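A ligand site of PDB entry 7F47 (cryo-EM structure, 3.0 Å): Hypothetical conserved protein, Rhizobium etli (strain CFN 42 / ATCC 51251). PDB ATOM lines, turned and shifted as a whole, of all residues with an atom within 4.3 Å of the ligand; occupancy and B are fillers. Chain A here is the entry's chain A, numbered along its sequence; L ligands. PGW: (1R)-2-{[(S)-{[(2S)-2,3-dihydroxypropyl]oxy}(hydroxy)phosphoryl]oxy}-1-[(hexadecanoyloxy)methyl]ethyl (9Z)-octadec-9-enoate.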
ATOM      1  N   PHE A  38       8.408  -9.227 -36.425  1.00  0.00           N
ATOM      2  CA  PHE A  38       7.125  -8.527 -36.193  1.00  0.00           C
ATOM      3  C   PHE A  38       6.680  -7.848 -37.497  1.00  0.00           C
ATOM      4  O   PHE A  38       5.518  -8.027 -37.887  1.00  0.00           O
ATOM      5  CB  PHE A  38       7.176  -7.487 -35.072  1.00  0.00           C
ATOM      6  CG  PHE A  38       5.815  -6.995 -34.679  1.00  0.00           C
ATOM      7  CD1 PHE A  38       4.905  -7.874 -34.102  1.00  0.00           C
ATOM      8  CD2 PHE A  38       5.395  -5.702 -34.947  1.00  0.00           C
ATOM      9  CE1 PHE A  38       3.631  -7.457 -33.770  1.00  0.00           C
ATOM     10  CE2 PHE A  38       4.113  -5.291 -34.611  1.00  0.00           C
ATOM     11  CZ  PHE A  38       3.236  -6.162 -34.019  1.00  0.00           C
ATOM     12  N   ILE A  45      -0.357 -10.569 -41.829  1.00  0.00           N
ATOM     13  CA  ILE A  45      -1.710 -10.467 -41.214  1.00  0.00           C
ATOM     14  C   ILE A  45      -2.534  -9.475 -42.032  1.00  0.00           C
ATOM     15  O   ILE A  45      -3.792  -9.597 -42.032  1.00  0.00           O
ATOM     16  CB  ILE A  45      -1.622 -10.075 -39.734  1.00  0.00           C
ATOM     17  CG1 ILE A  45      -2.660 -10.849 -38.923  1.00  0.00           C
ATOM     18  CG2 ILE A  45      -1.747  -8.573 -39.562  1.00  0.00           C
ATOM     19  CD1 ILE A  45      -2.560 -10.642 -37.443  1.00  0.00           C
ATOM     20  N   THR A 116       1.960 -11.326 -20.533  1.00  0.00           N
ATOM     21  CA  THR A 116       1.629 -10.021 -21.163  1.00  0.00           C
ATOM     22  C   THR A 116       2.920  -9.405 -21.709  1.00  0.00           C
ATOM     23  O   THR A 116       2.803  -8.727 -22.729  1.00  0.00           O
ATOM     24  CB  THR A 116       0.904  -9.090 -20.193  1.00  0.00           C
ATOM     25  OG1 THR A 116       1.401  -9.212 -18.853  1.00  0.00           O
ATOM     26  CG2 THR A 116      -0.572  -9.398 -20.187  1.00  0.00           C
ATOM     27  N   PRO A 271       6.745  -9.277 -27.529  1.00  0.00           N
ATOM     28  CA  PRO A 271       5.947  -9.253 -26.309  1.00  0.00           C
ATOM     29  C   PRO A 271       4.567  -9.918 -26.466  1.00  0.00           C
ATOM     30  O   PRO A 271       3.867  -9.580 -27.400  1.00  0.00           O
ATOM     31  CB  PRO A 271       5.748  -7.751 -26.033  1.00  0.00           C
ATOM     32  CG  PRO A 271       6.977  -7.114 -26.630  1.00  0.00           C
ATOM     33  CD  PRO A 271       7.325  -7.958 -27.836  1.00  0.00           C
ATOM     34  N   ALA A 272       4.251 -10.924 -25.643  1.00  0.00           N
ATOM     35  CA  ALA A 272       2.979 -11.693 -25.682  1.00  0.00           C
ATOM     36  C   ALA A 272       2.787 -12.498 -26.975  1.00  0.00           C
ATOM     37  O   ALA A 272       1.676 -12.991 -27.164  1.00  0.00           O
ATOM     38  CB  ALA A 272       1.823 -10.742 -25.529  1.00  0.00           C
ATOM     39  N   LEU A 274       2.633 -10.948 -29.940  1.00  0.00           N
ATOM     40  CA  LEU A 274       1.470 -10.113 -30.324  1.00  0.00           C
ATOM     41  C   LEU A 274       1.040 -10.426 -31.767  1.00  0.00           C
ATOM     42  O   LEU A 274      -0.169 -10.646 -31.942  1.00  0.00           O
ATOM     43  CB  LEU A 274       1.762  -8.613 -30.156  1.00  0.00           C
ATOM     44  CG  LEU A 274       0.563  -7.716 -30.454  1.00  0.00           C
ATOM     45  CD1 LEU A 274      -0.685  -8.161 -29.675  1.00  0.00           C
ATOM     46  CD2 LEU A 274       0.940  -6.265 -30.206  1.00  0.00           C
ATOM     47  N   GLU A 278      -1.518 -14.387 -33.567  1.00  0.00           N
ATOM     48  CA  GLU A 278      -2.727 -14.115 -34.390  1.00  0.00           C
ATOM     49  C   GLU A 278      -2.484 -14.618 -35.829  1.00  0.00           C
ATOM     50  O   GLU A 278      -3.442 -15.103 -36.440  1.00  0.00           O
ATOM     51  CB  GLU A 278      -3.119 -12.633 -34.475  1.00  0.00           C
ATOM     52  CG  GLU A 278      -2.602 -11.754 -33.357  1.00  0.00           C
ATOM     53  CD  GLU A 278      -3.132 -12.011 -31.951  1.00  0.00           C
ATOM     54  OE1 GLU A 278      -2.335 -12.382 -31.081  1.00  0.00           O
ATOM     55  OE2 GLU A 278      -4.355 -11.851 -31.734  1.00  0.00           O
ATOM     56  N   VAL A 299      -9.406 -11.025 -30.310  1.00  0.00           N
ATOM     57  CA  VAL A 299      -9.470  -9.796 -29.464  1.00  0.00           C
ATOM     58  C   VAL A 299      -9.880 -10.215 -28.058  1.00  0.00           C
ATOM     59  O   VAL A 299      -9.183  -9.836 -27.098  1.00  0.00           O
ATOM     60  CB  VAL A 299     -10.454  -8.756 -30.008  1.00  0.00           C
ATOM     61  CG1 VAL A 299     -10.719  -7.682 -28.977  1.00  0.00           C
ATOM     62  CG2 VAL A 299      -9.970  -8.126 -31.286  1.00  0.00           C
ATOM     63  N   ARG A 302      -7.295 -12.123 -25.982  1.00  0.00           N
ATOM     64  CA  ARG A 302      -6.230 -11.230 -25.449  1.00  0.00           C
ATOM     65  C   ARG A 302      -6.797 -10.427 -24.289  1.00  0.00           C
ATOM     66  O   ARG A 302      -6.016 -10.158 -23.346  1.00  0.00           O
ATOM     67  CB  ARG A 302      -5.688 -10.295 -26.535  1.00  0.00           C
ATOM     68  CG  ARG A 302      -4.901 -11.063 -27.588  1.00  0.00           C
ATOM     69  CD  ARG A 302      -3.485 -10.583 -27.710  1.00  0.00           C
ATOM     70  NE  ARG A 302      -2.660 -11.468 -28.484  1.00  0.00           N
ATOM     71  CZ  ARG A 302      -1.635 -12.149 -28.002  1.00  0.00           C
ATOM     72  NH1 ARG A 302      -1.291 -12.067 -26.731  1.00  0.00           N
ATOM     73  NH2 ARG A 302      -0.912 -12.886 -28.829  1.00  0.00           N
ATOM     74  N   LEU A 303      -8.090 -10.096 -24.294  1.00  0.00           N
ATOM     75  CA  LEU A 303      -8.697  -9.406 -23.110  1.00  0.00           C
ATOM     76  C   LEU A 303      -8.766 -10.362 -21.935  1.00  0.00           C
ATOM     77  O   LEU A 303      -8.281 -10.007 -20.850  1.00  0.00           O
ATOM     78  CB  LEU A 303     -10.108  -8.901 -23.413  1.00  0.00           C
ATOM     79  CG  LEU A 303     -10.152  -7.684 -24.341  1.00  0.00           C
ATOM     80  CD1 LEU A 303     -11.466  -6.962 -24.133  1.00  0.00           C
ATOM     81  CD2 LEU A 303      -8.972  -6.727 -24.131  1.00  0.00           C
ATOM     82  N   VAL A 307      -5.209  -9.443 -20.346  1.00  0.00           N
ATOM     83  CA  VAL A 307      -5.486  -8.150 -19.658  1.00  0.00           C
ATOM     84  C   VAL A 307      -6.176  -8.420 -18.324  1.00  0.00           C
ATOM     85  O   VAL A 307      -5.927  -7.690 -17.371  1.00  0.00           O
ATOM     86  CB  VAL A 307      -6.342  -7.254 -20.530  1.00  0.00           C
ATOM     87  CG1 VAL A 307      -6.763  -5.995 -19.755  1.00  0.00           C
ATOM     88  CG2 VAL A 307      -5.612  -6.949 -21.824  1.00  0.00           C
ATOM     89  N   LEU A 351       1.801  -0.149 -18.971  1.00  0.00           N
ATOM     90  CA  LEU A 351       2.222  -0.469 -20.350  1.00  0.00           C
ATOM     91  C   LEU A 351       0.987  -0.897 -21.162  1.00  0.00           C
ATOM     92  O   LEU A 351       0.778  -0.299 -22.226  1.00  0.00           O
ATOM     93  CB  LEU A 351       3.296  -1.538 -20.261  1.00  0.00           C
ATOM     94  CG  LEU A 351       3.709  -2.131 -21.577  1.00  0.00           C
ATOM     95  CD1 LEU A 351       4.791  -1.320 -22.227  1.00  0.00           C
ATOM     96  CD2 LEU A 351       4.183  -3.541 -21.340  1.00  0.00           C
ATOM     97  N   LEU A 352       0.128  -1.783 -20.647  1.00  0.00           N
ATOM     98  CA  LEU A 352      -1.125  -2.197 -21.357  1.00  0.00           C
ATOM     99  C   LEU A 352      -2.011  -0.983 -21.622  1.00  0.00           C
ATOM    100  O   LEU A 352      -2.502  -0.885 -22.733  1.00  0.00           O
ATOM    101  CB  LEU A 352      -1.905  -3.247 -20.551  1.00  0.00           C
ATOM    102  CG  LEU A 352      -1.307  -4.653 -20.605  1.00  0.00           C
ATOM    103  CD1 LEU A 352      -2.164  -5.671 -19.863  1.00  0.00           C
ATOM    104  CD2 LEU A 352      -1.078  -5.094 -22.036  1.00  0.00           C
ATOM    105  N   VAL A 355      -0.567   0.949 -24.533  1.00  0.00           N
ATOM    106  CA  VAL A 355      -0.947   0.199 -25.768  1.00  0.00           C
ATOM    107  C   VAL A 355      -2.398   0.546 -26.079  1.00  0.00           C
ATOM    108  O   VAL A 355      -2.662   0.959 -27.232  1.00  0.00           O
ATOM    109  CB  VAL A 355      -0.794  -1.315 -25.614  1.00  0.00           C
ATOM    110  CG1 VAL A 355      -1.022  -2.047 -26.919  1.00  0.00           C
ATOM    111  CG2 VAL A 355       0.554  -1.673 -25.030  1.00  0.00           C
ATOM    112  N   MET A 356      -3.297   0.450 -25.102  1.00  0.00           N
ATOM    113  CA  MET A 356      -4.741   0.718 -25.318  1.00  0.00           C
ATOM    114  C   MET A 356      -4.902   2.105 -25.935  1.00  0.00           C
ATOM    115  O   MET A 356      -5.571   2.199 -26.979  1.00  0.00           O
ATOM    116  CB  MET A 356      -5.535   0.678 -24.011  1.00  0.00           C
ATOM    117  CG  MET A 356      -6.968   1.127 -24.169  1.00  0.00           C
ATOM    118  SD  MET A 356      -7.856   1.117 -22.615  1.00  0.00           S
ATOM    119  CE  MET A 356      -7.092   2.510 -21.785  1.00  0.00           C
ATOM    120  N   PHE A 359      -3.607   2.337 -29.635  1.00  0.00           N
ATOM    121  CA  PHE A 359      -4.444   1.514 -30.549  1.00  0.00           C
ATOM    122  C   PHE A 359      -5.811   2.180 -30.722  1.00  0.00           C
ATOM    123  O   PHE A 359      -6.332   2.184 -31.862  1.00  0.00           O
ATOM    124  CB  PHE A 359      -4.566   0.079 -30.045  1.00  0.00           C
ATOM    125  CG  PHE A 359      -3.327  -0.749 -30.277  1.00  0.00           C
ATOM    126  CD1 PHE A 359      -2.125  -0.166 -30.713  1.00  0.00           C
ATOM    127  CD2 PHE A 359      -3.334  -2.110 -29.994  1.00  0.00           C
ATOM    128  CE1 PHE A 359      -0.996  -0.936 -30.918  1.00  0.00           C
ATOM    129  CE2 PHE A 359      -2.195  -2.867 -30.167  1.00  0.00           C
ATOM    130  CZ  PHE A 359      -1.030  -2.283 -30.640  1.00  0.00           C
ATOM    131  N   SER A 360      -6.352   2.741 -29.655  1.00  0.00           N
ATOM    132  CA  SER A 360      -7.684   3.394 -29.695  1.00  0.00           C
ATOM    133  C   SER A 360      -7.556   4.628 -30.570  1.00  0.00           C
ATOM    134  O   SER A 360      -8.573   5.042 -31.137  1.00  0.00           O
ATOM    135  CB  SER A 360      -8.201   3.738 -28.330  1.00  0.00           C
ATOM    136  OG  SER A 360      -7.918   5.091 -28.016  1.00  0.00           O
ATOM    137  N   THR A 363      -8.007   3.554 -34.060  1.00  0.00           N
ATOM    138  CA  THR A 363      -9.242   2.763 -34.292  1.00  0.00           C
ATOM    139  C   THR A 363     -10.445   3.696 -34.394  1.00  0.00           C
ATOM    140  O   THR A 363     -10.495   4.734 -33.737  1.00  0.00           O
ATOM    141  CB  THR A 363      -9.360   1.664 -33.215  1.00  0.00           C
ATOM    142  OG1 THR A 363      -9.197   0.381 -33.806  1.00  0.00           O
ATOM    143  CG2 THR A 363     -10.682   1.688 -32.486  1.00  0.00           C
ATOM    144  N   PRO A 364     -11.471   3.368 -35.219  1.00  0.00           N
ATOM    145  CA  PRO A 364     -12.680   4.185 -35.359  1.00  0.00           C
ATOM    146  C   PRO A 364     -13.523   4.258 -34.085  1.00  0.00           C
ATOM    147  O   PRO A 364     -13.628   3.231 -33.419  1.00  0.00           O
ATOM    148  CB  PRO A 364     -13.508   3.430 -36.380  1.00  0.00           C
ATOM    149  CG  PRO A 364     -12.477   2.682 -37.172  1.00  0.00           C
ATOM    150  CD  PRO A 364     -11.498   2.211 -36.125  1.00  0.00           C
ATOM    151  N   THR A 365     -14.099   5.424 -33.811  1.00  0.00           N
ATOM    152  CA  THR A 365     -15.102   5.663 -32.732  1.00  0.00           C
ATOM    153  C   THR A 365     -16.512   5.511 -33.311  1.00  0.00           C
ATOM    154  O   THR A 365     -16.732   5.817 -34.476  1.00  0.00           O
ATOM    155  CB  THR A 365     -14.954   7.038 -32.067  1.00  0.00           C
ATOM    156  OG1 THR A 365     -16.127   7.273 -31.289  1.00  0.00           O
ATOM    157  CG2 THR A 365     -14.802   8.167 -33.051  1.00  0.00           C
ATOM    158  N   LYS A 428     -13.187  12.764 -26.489  1.00  0.00           N
ATOM    159  CA  LYS A 428     -12.840  12.433 -27.890  1.00  0.00           C
ATOM    160  C   LYS A 428     -13.771  11.338 -28.402  1.00  0.00           C
ATOM    161  O   LYS A 428     -13.906  11.278 -29.647  1.00  0.00           O
ATOM    162  CB  LYS A 428     -11.368  12.002 -28.006  1.00  0.00           C
ATOM    163  CG  LYS A 428     -11.026  10.611 -27.485  1.00  0.00           C
ATOM    164  CD  LYS A 428      -9.808  10.024 -28.138  1.00  0.00           C
ATOM    165  CE  LYS A 428      -9.807   8.508 -28.098  1.00  0.00           C
ATOM    166  NZ  LYS A 428      -9.773   8.008 -26.703  1.00  0.00           N
ATOM    167  N   ALA A 429     -14.334  10.483 -27.550  1.00  0.00           N
ATOM    168  CA  ALA A 429     -15.213   9.406 -28.049  1.00  0.00           C
ATOM    169  C   ALA A 429     -16.193   8.887 -26.991  1.00  0.00           C
ATOM    170  O   ALA A 429     -16.771   7.793 -27.224  1.00  0.00           O
ATOM    171  CB  ALA A 429     -14.336   8.281 -28.574  1.00  0.00           C
ATOM    172  N   ALA A 431     -15.535   7.450 -24.313  1.00  0.00           N
ATOM    173  CA  ALA A 431     -14.942   6.085 -24.232  1.00  0.00           C
ATOM    174  C   ALA A 431     -14.976   5.618 -22.771  1.00  0.00           C
ATOM    175  O   ALA A 431     -13.943   5.678 -22.080  1.00  0.00           O
ATOM    176  CB  ALA A 431     -13.542   6.069 -24.780  1.00  0.00           C
ATOM    177  N   LEU A 432     -16.142   5.128 -22.346  1.00  0.00           N
ATOM    178  CA  LEU A 432     -16.442   4.769 -20.936  1.00  0.00           C
ATOM    179  C   LEU A 432     -15.537   3.614 -20.501  1.00  0.00           C
ATOM    180  O   LEU A 432     -14.988   3.698 -19.392  1.00  0.00           O
ATOM    181  CB  LEU A 432     -17.915   4.391 -20.806  1.00  0.00           C
ATOM    182  CG  LEU A 432     -18.921   5.494 -21.151  1.00  0.00           C
ATOM    183  CD1 LEU A 432     -20.312   5.105 -20.697  1.00  0.00           C
ATOM    184  CD2 LEU A 432     -18.516   6.832 -20.542  1.00  0.00           C
ATOM    185  N   VAL A 433     -15.327   2.611 -21.357  1.00  0.00           N
ATOM    186  CA  VAL A 433     -14.545   1.398 -20.966  1.00  0.00           C
ATOM    187  C   VAL A 433     -13.062   1.789 -20.815  1.00  0.00           C
ATOM    188  O   VAL A 433     -12.394   1.276 -19.896  1.00  0.00           O
ATOM    189  CB  VAL A 433     -14.708   0.229 -21.950  1.00  0.00           C
ATOM    190  CG1 VAL A 433     -14.684  -1.098 -21.211  1.00  0.00           C
ATOM    191  CG2 VAL A 433     -15.966   0.330 -22.788  1.00  0.00           C
ATOM    192  N   GLU A 434     -12.554   2.702 -21.642  1.00  0.00           N
ATOM    193  CA  GLU A 434     -11.154   3.171 -21.530  1.00  0.00           C
ATOM    194  C   GLU A 434     -11.050   3.977 -20.247  1.00  0.00           C
ATOM    195  O   GLU A 434     -10.078   3.747 -19.507  1.00  0.00           O
ATOM    196  CB  GLU A 434     -10.732   4.016 -22.717  1.00  0.00           C
ATOM    197  CG  GLU A 434     -10.815   3.242 -23.997  1.00  0.00           C
ATOM    198  CD  GLU A 434     -10.300   3.967 -25.221  1.00  0.00           C
ATOM    199  OE1 GLU A 434      -9.399   4.810 -25.061  1.00  0.00           O
ATOM    200  OE2 GLU A 434     -10.792   3.679 -26.327  1.00  0.00           O
ATOM    201  N   PHE A 437     -10.775   1.586 -17.288  1.00  0.00           N
ATOM    202  CA  PHE A 437      -9.439   0.942 -17.163  1.00  0.00           C
ATOM    203  C   PHE A 437      -8.482   1.966 -16.556  1.00  0.00           C
ATOM    204  O   PHE A 437      -7.740   1.653 -15.636  1.00  0.00           O
ATOM    205  CB  PHE A 437      -9.001   0.377 -18.516  1.00  0.00           C
ATOM    206  CG  PHE A 437      -9.565  -0.985 -18.801  1.00  0.00           C
ATOM    207  CD1 PHE A 437     -10.915  -1.226 -18.691  1.00  0.00           C
ATOM    208  CD2 PHE A 437      -8.744  -2.046 -19.138  1.00  0.00           C
ATOM    209  CE1 PHE A 437     -11.445  -2.479 -18.946  1.00  0.00           C
ATOM    210  CE2 PHE A 437      -9.278  -3.291 -19.415  1.00  0.00           C
ATOM    211  CZ  PHE A 437     -10.627  -3.504 -19.313  1.00  0.00           C
ATOM    212  N   ALA A 470       9.787  -2.952 -27.575  1.00  0.00           N
ATOM    213  CA  ALA A 470       8.356  -2.948 -27.205  1.00  0.00           C
ATOM    214  C   ALA A 470       7.686  -1.695 -27.796  1.00  0.00           C
ATOM    215  O   ALA A 470       6.638  -1.845 -28.440  1.00  0.00           O
ATOM    216  CB  ALA A 470       8.163  -3.009 -25.715  1.00  0.00           C
ATOM    217  N   VAL A 473       7.269  -2.274 -31.534  1.00  0.00           N
ATOM    218  CA  VAL A 473       6.137  -3.190 -31.909  1.00  0.00           C
ATOM    219  C   VAL A 473       4.841  -2.421 -31.683  1.00  0.00           C
ATOM    220  O   VAL A 473       3.951  -2.536 -32.548  1.00  0.00           O
ATOM    221  CB  VAL A 473       6.116  -4.572 -31.222  1.00  0.00           C
ATOM    222  CG1 VAL A 473       7.446  -5.282 -31.365  1.00  0.00           C
ATOM    223  CG2 VAL A 473       5.706  -4.545 -29.772  1.00  0.00           C
ATOM    224  N   ILE A 474       4.733  -1.627 -30.622  1.00  0.00           N
ATOM    225  CA  ILE A 474       3.500  -0.822 -30.385  1.00  0.00           C
ATOM    226  C   ILE A 474       3.262   0.122 -31.575  1.00  0.00           C
ATOM    227  O   ILE A 474       2.120   0.220 -32.049  1.00  0.00           O
ATOM    228  CB  ILE A 474       3.625  -0.079 -29.053  1.00  0.00           C
ATOM    229  CG1 ILE A 474       3.417  -1.088 -27.922  1.00  0.00           C
ATOM    230  CG2 ILE A 474       2.670   1.117 -28.996  1.00  0.00           C
ATOM    231  CD1 ILE A 474       3.739  -0.560 -26.529  1.00  0.00           C
ATOM    232  N   VAL A 480      -0.163  -1.127 -38.697  1.00  0.00           N
ATOM    233  CA  VAL A 480      -0.964  -2.275 -39.200  1.00  0.00           C
ATOM    234  C   VAL A 480      -2.454  -2.053 -38.866  1.00  0.00           C
ATOM    235  O   VAL A 480      -3.312  -2.206 -39.748  1.00  0.00           O
ATOM    236  CB  VAL A 480      -0.468  -3.601 -38.619  1.00  0.00           C
ATOM    237  CG1 VAL A 480      -1.415  -4.764 -38.881  1.00  0.00           C
ATOM    238  CG2 VAL A 480       0.910  -3.918 -39.160  1.00  0.00           C
HETATM  239  CAD PGW L   1     -12.780   4.331 -28.594  1.00  0.00           C
HETATM  240  OAE PGW L   1     -11.537   4.929 -28.946  1.00  0.00           O
HETATM  241  OAF PGW L   1     -12.650   2.981 -30.542  1.00  0.00           O
HETATM  242  P   PGW L   1     -14.952   2.104 -26.321  1.00  0.00           P
HETATM  243  C01 PGW L   1     -10.342   0.117 -26.069  1.00  0.00           C
HETATM  244  C1  PGW L   1     -11.745  -1.861 -24.416  1.00  0.00           C
HETATM  245  O01 PGW L   1     -12.074  -1.575 -25.691  1.00  0.00           O
HETATM  246  C02 PGW L   1     -11.797  -0.253 -26.263  1.00  0.00           C
HETATM  247  C2  PGW L   1     -10.460  -2.616 -24.259  1.00  0.00           C
HETATM  248  O02 PGW L   1     -12.435  -1.595 -23.474  1.00  0.00           O
HETATM  249  C03 PGW L   1     -12.745   0.775 -25.676  1.00  0.00           C
HETATM  250  C3  PGW L   1      -9.599  -2.065 -23.181  1.00  0.00           C
HETATM  251  O03 PGW L   1      -9.841   0.782 -27.254  1.00  0.00           O
HETATM  252  C04 PGW L   1     -14.188   2.219 -28.879  1.00  0.00           C
HETATM  253  C4  PGW L   1      -8.363  -2.907 -22.915  1.00  0.00           C
HETATM  254  O04 PGW L   1     -10.347  -0.118 -29.218  1.00  0.00           O
HETATM  255  C05 PGW L   1     -12.874   2.924 -29.141  1.00  0.00           C
HETATM  256  C5  PGW L   1      -7.118  -2.392 -23.592  1.00  0.00           C
HETATM  257  C06 PGW L   1      -3.006  -7.111 -26.315  1.00  0.00           C
HETATM  258  C6  PGW L   1      -5.831  -2.984 -23.074  1.00  0.00           C
HETATM  259  C07 PGW L   1      -2.184  -7.849 -25.282  1.00  0.00           C
HETATM  260  C7  PGW L   1      -5.283  -4.130 -23.912  1.00  0.00           C
HETATM  261  C08 PGW L   1      -0.681  -7.772 -25.480  1.00  0.00           C
HETATM  262  C8  PGW L   1      -4.392  -3.700 -25.043  1.00  0.00           C
HETATM  263  C09 PGW L   1      -0.121  -6.379 -25.661  1.00  0.00           C
HETATM  264  C9  PGW L   1      -3.865  -4.812 -25.897  1.00  0.00           C
HETATM  265  C10 PGW L   1      -3.921  -6.098 -25.692  1.00  0.00           C
HETATM  266  C11 PGW L   1       1.270  -6.208 -25.090  1.00  0.00           C
HETATM  267  O11 PGW L   1     -13.976   0.835 -26.454  1.00  0.00           O
HETATM  268  C12 PGW L   1       2.189  -5.361 -25.915  1.00  0.00           C
HETATM  269  O12 PGW L   1     -14.909   2.818 -27.763  1.00  0.00           O
HETATM  270  C13 PGW L   1       3.400  -4.884 -25.153  1.00  0.00           C
HETATM  271  O13 PGW L   1     -14.351   3.069 -25.325  1.00  0.00           O
HETATM  272  C14 PGW L   1       4.579  -4.468 -26.010  1.00  0.00           C
HETATM  273  O14 PGW L   1     -16.363   1.611 -26.117  1.00  0.00           O
HETATM  274  C15 PGW L   1      -5.751  -8.535 -31.816  1.00  0.00           C
HETATM  275  C16 PGW L   1      -5.061  -9.108 -33.042  1.00  0.00           C
HETATM  276  C17 PGW L   1      -4.304  -8.097 -33.887  1.00  0.00           C
HETATM  277  C18 PGW L   1      -2.803  -8.050 -33.626  1.00  0.00           C
HETATM  278  C19 PGW L   1      -9.579   0.007 -28.312  1.00  0.00           C
HETATM  279  C20 PGW L   1      -8.254  -0.701 -28.214  1.00  0.00           C
HETATM  280  C21 PGW L   1      -8.300  -2.140 -28.677  1.00  0.00           C
HETATM  281  C22 PGW L   1      -7.421  -3.059 -27.862  1.00  0.00           C
HETATM  282  C23 PGW L   1      -7.509  -4.535 -28.237  1.00  0.00           C
HETATM  283  C24 PGW L   1      -6.712  -4.938 -29.465  1.00  0.00           C
HETATM  284  C25 PGW L   1      -5.896  -6.210 -29.295  1.00  0.00           C
HETATM  285  C26 PGW L   1      -4.968  -6.527 -30.456  1.00  0.00           C
HETATM  286  C27 PGW L   1      -4.829  -8.006 -30.735  1.00  0.00           C
HETATM  287  C28 PGW L   1      -2.168  -6.680 -33.691  1.00  0.00           C
HETATM  288  C29 PGW L   1      -1.175  -6.484 -35.979  1.00  0.00           C
HETATM  289  C30 PGW L   1      -0.914  -6.609 -34.506  1.00  0.00           C
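The guanidinium group (NH2) of Arg 302 lies within salt-bridge range of the side-chain carboxylate (OE1) of Glu 278 (2.7 Å).
The guanidinium group of Arg 302 lies within hydrogen-bond range of the backbone carbonyl oxygen of Ala 272, 3.1 Å away.
OE1 of Glu 434 is in salt-bridge range of NZ of Lys 428, 3.6 Å away.
The backbone carbonyl oxygen (O) of Arg 302 lies within hydrogen-bond range of the backbone NH (N) of Val 307.
The side-chain carboxylate (OE1) of Glu 434 sits at hydrogen-bond distance from the side-chain hydroxyl (OG) of Ser 360, 3.3 Å away.
Merely in contact with the ligand: Thr 116 (3.8 Å), Pro 271 (3.5 Å), Ala 272 (3.9 Å), Glu 278 (3.1 Å), Arg 302 (3.8 Å), Val 307 (3.5 Å), Leu 352 (3.95 Å), Met 356 (3.5 Å), Ser 360 (3.5 Å), Thr 363 (3.1 Å), Ala 431 (3.2 Å), Val 433 (3.2 Å), Phe 437 (3.6 Å), Ala 470 (3.9 Å), Val 473 (3.9 Å) and Val 480 (3.4 Å).
Hydrophobic or aromatic side chains that line the ligand: Pro 271, Ala 272, Val 307, Leu 352, Met 356, Ala 431, Val 433, Phe 437, Ala 470, Val 473 and Val 480.
Of the 31 residues printed, 18 come within 4 Å of the ligand.
O of Pro 364 is in hydrogen-bond range of OAF of the ligand, at 3.0 Å.
OE2 of Glu 434 is in hydrogen-bond range of OAE of the ligand.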
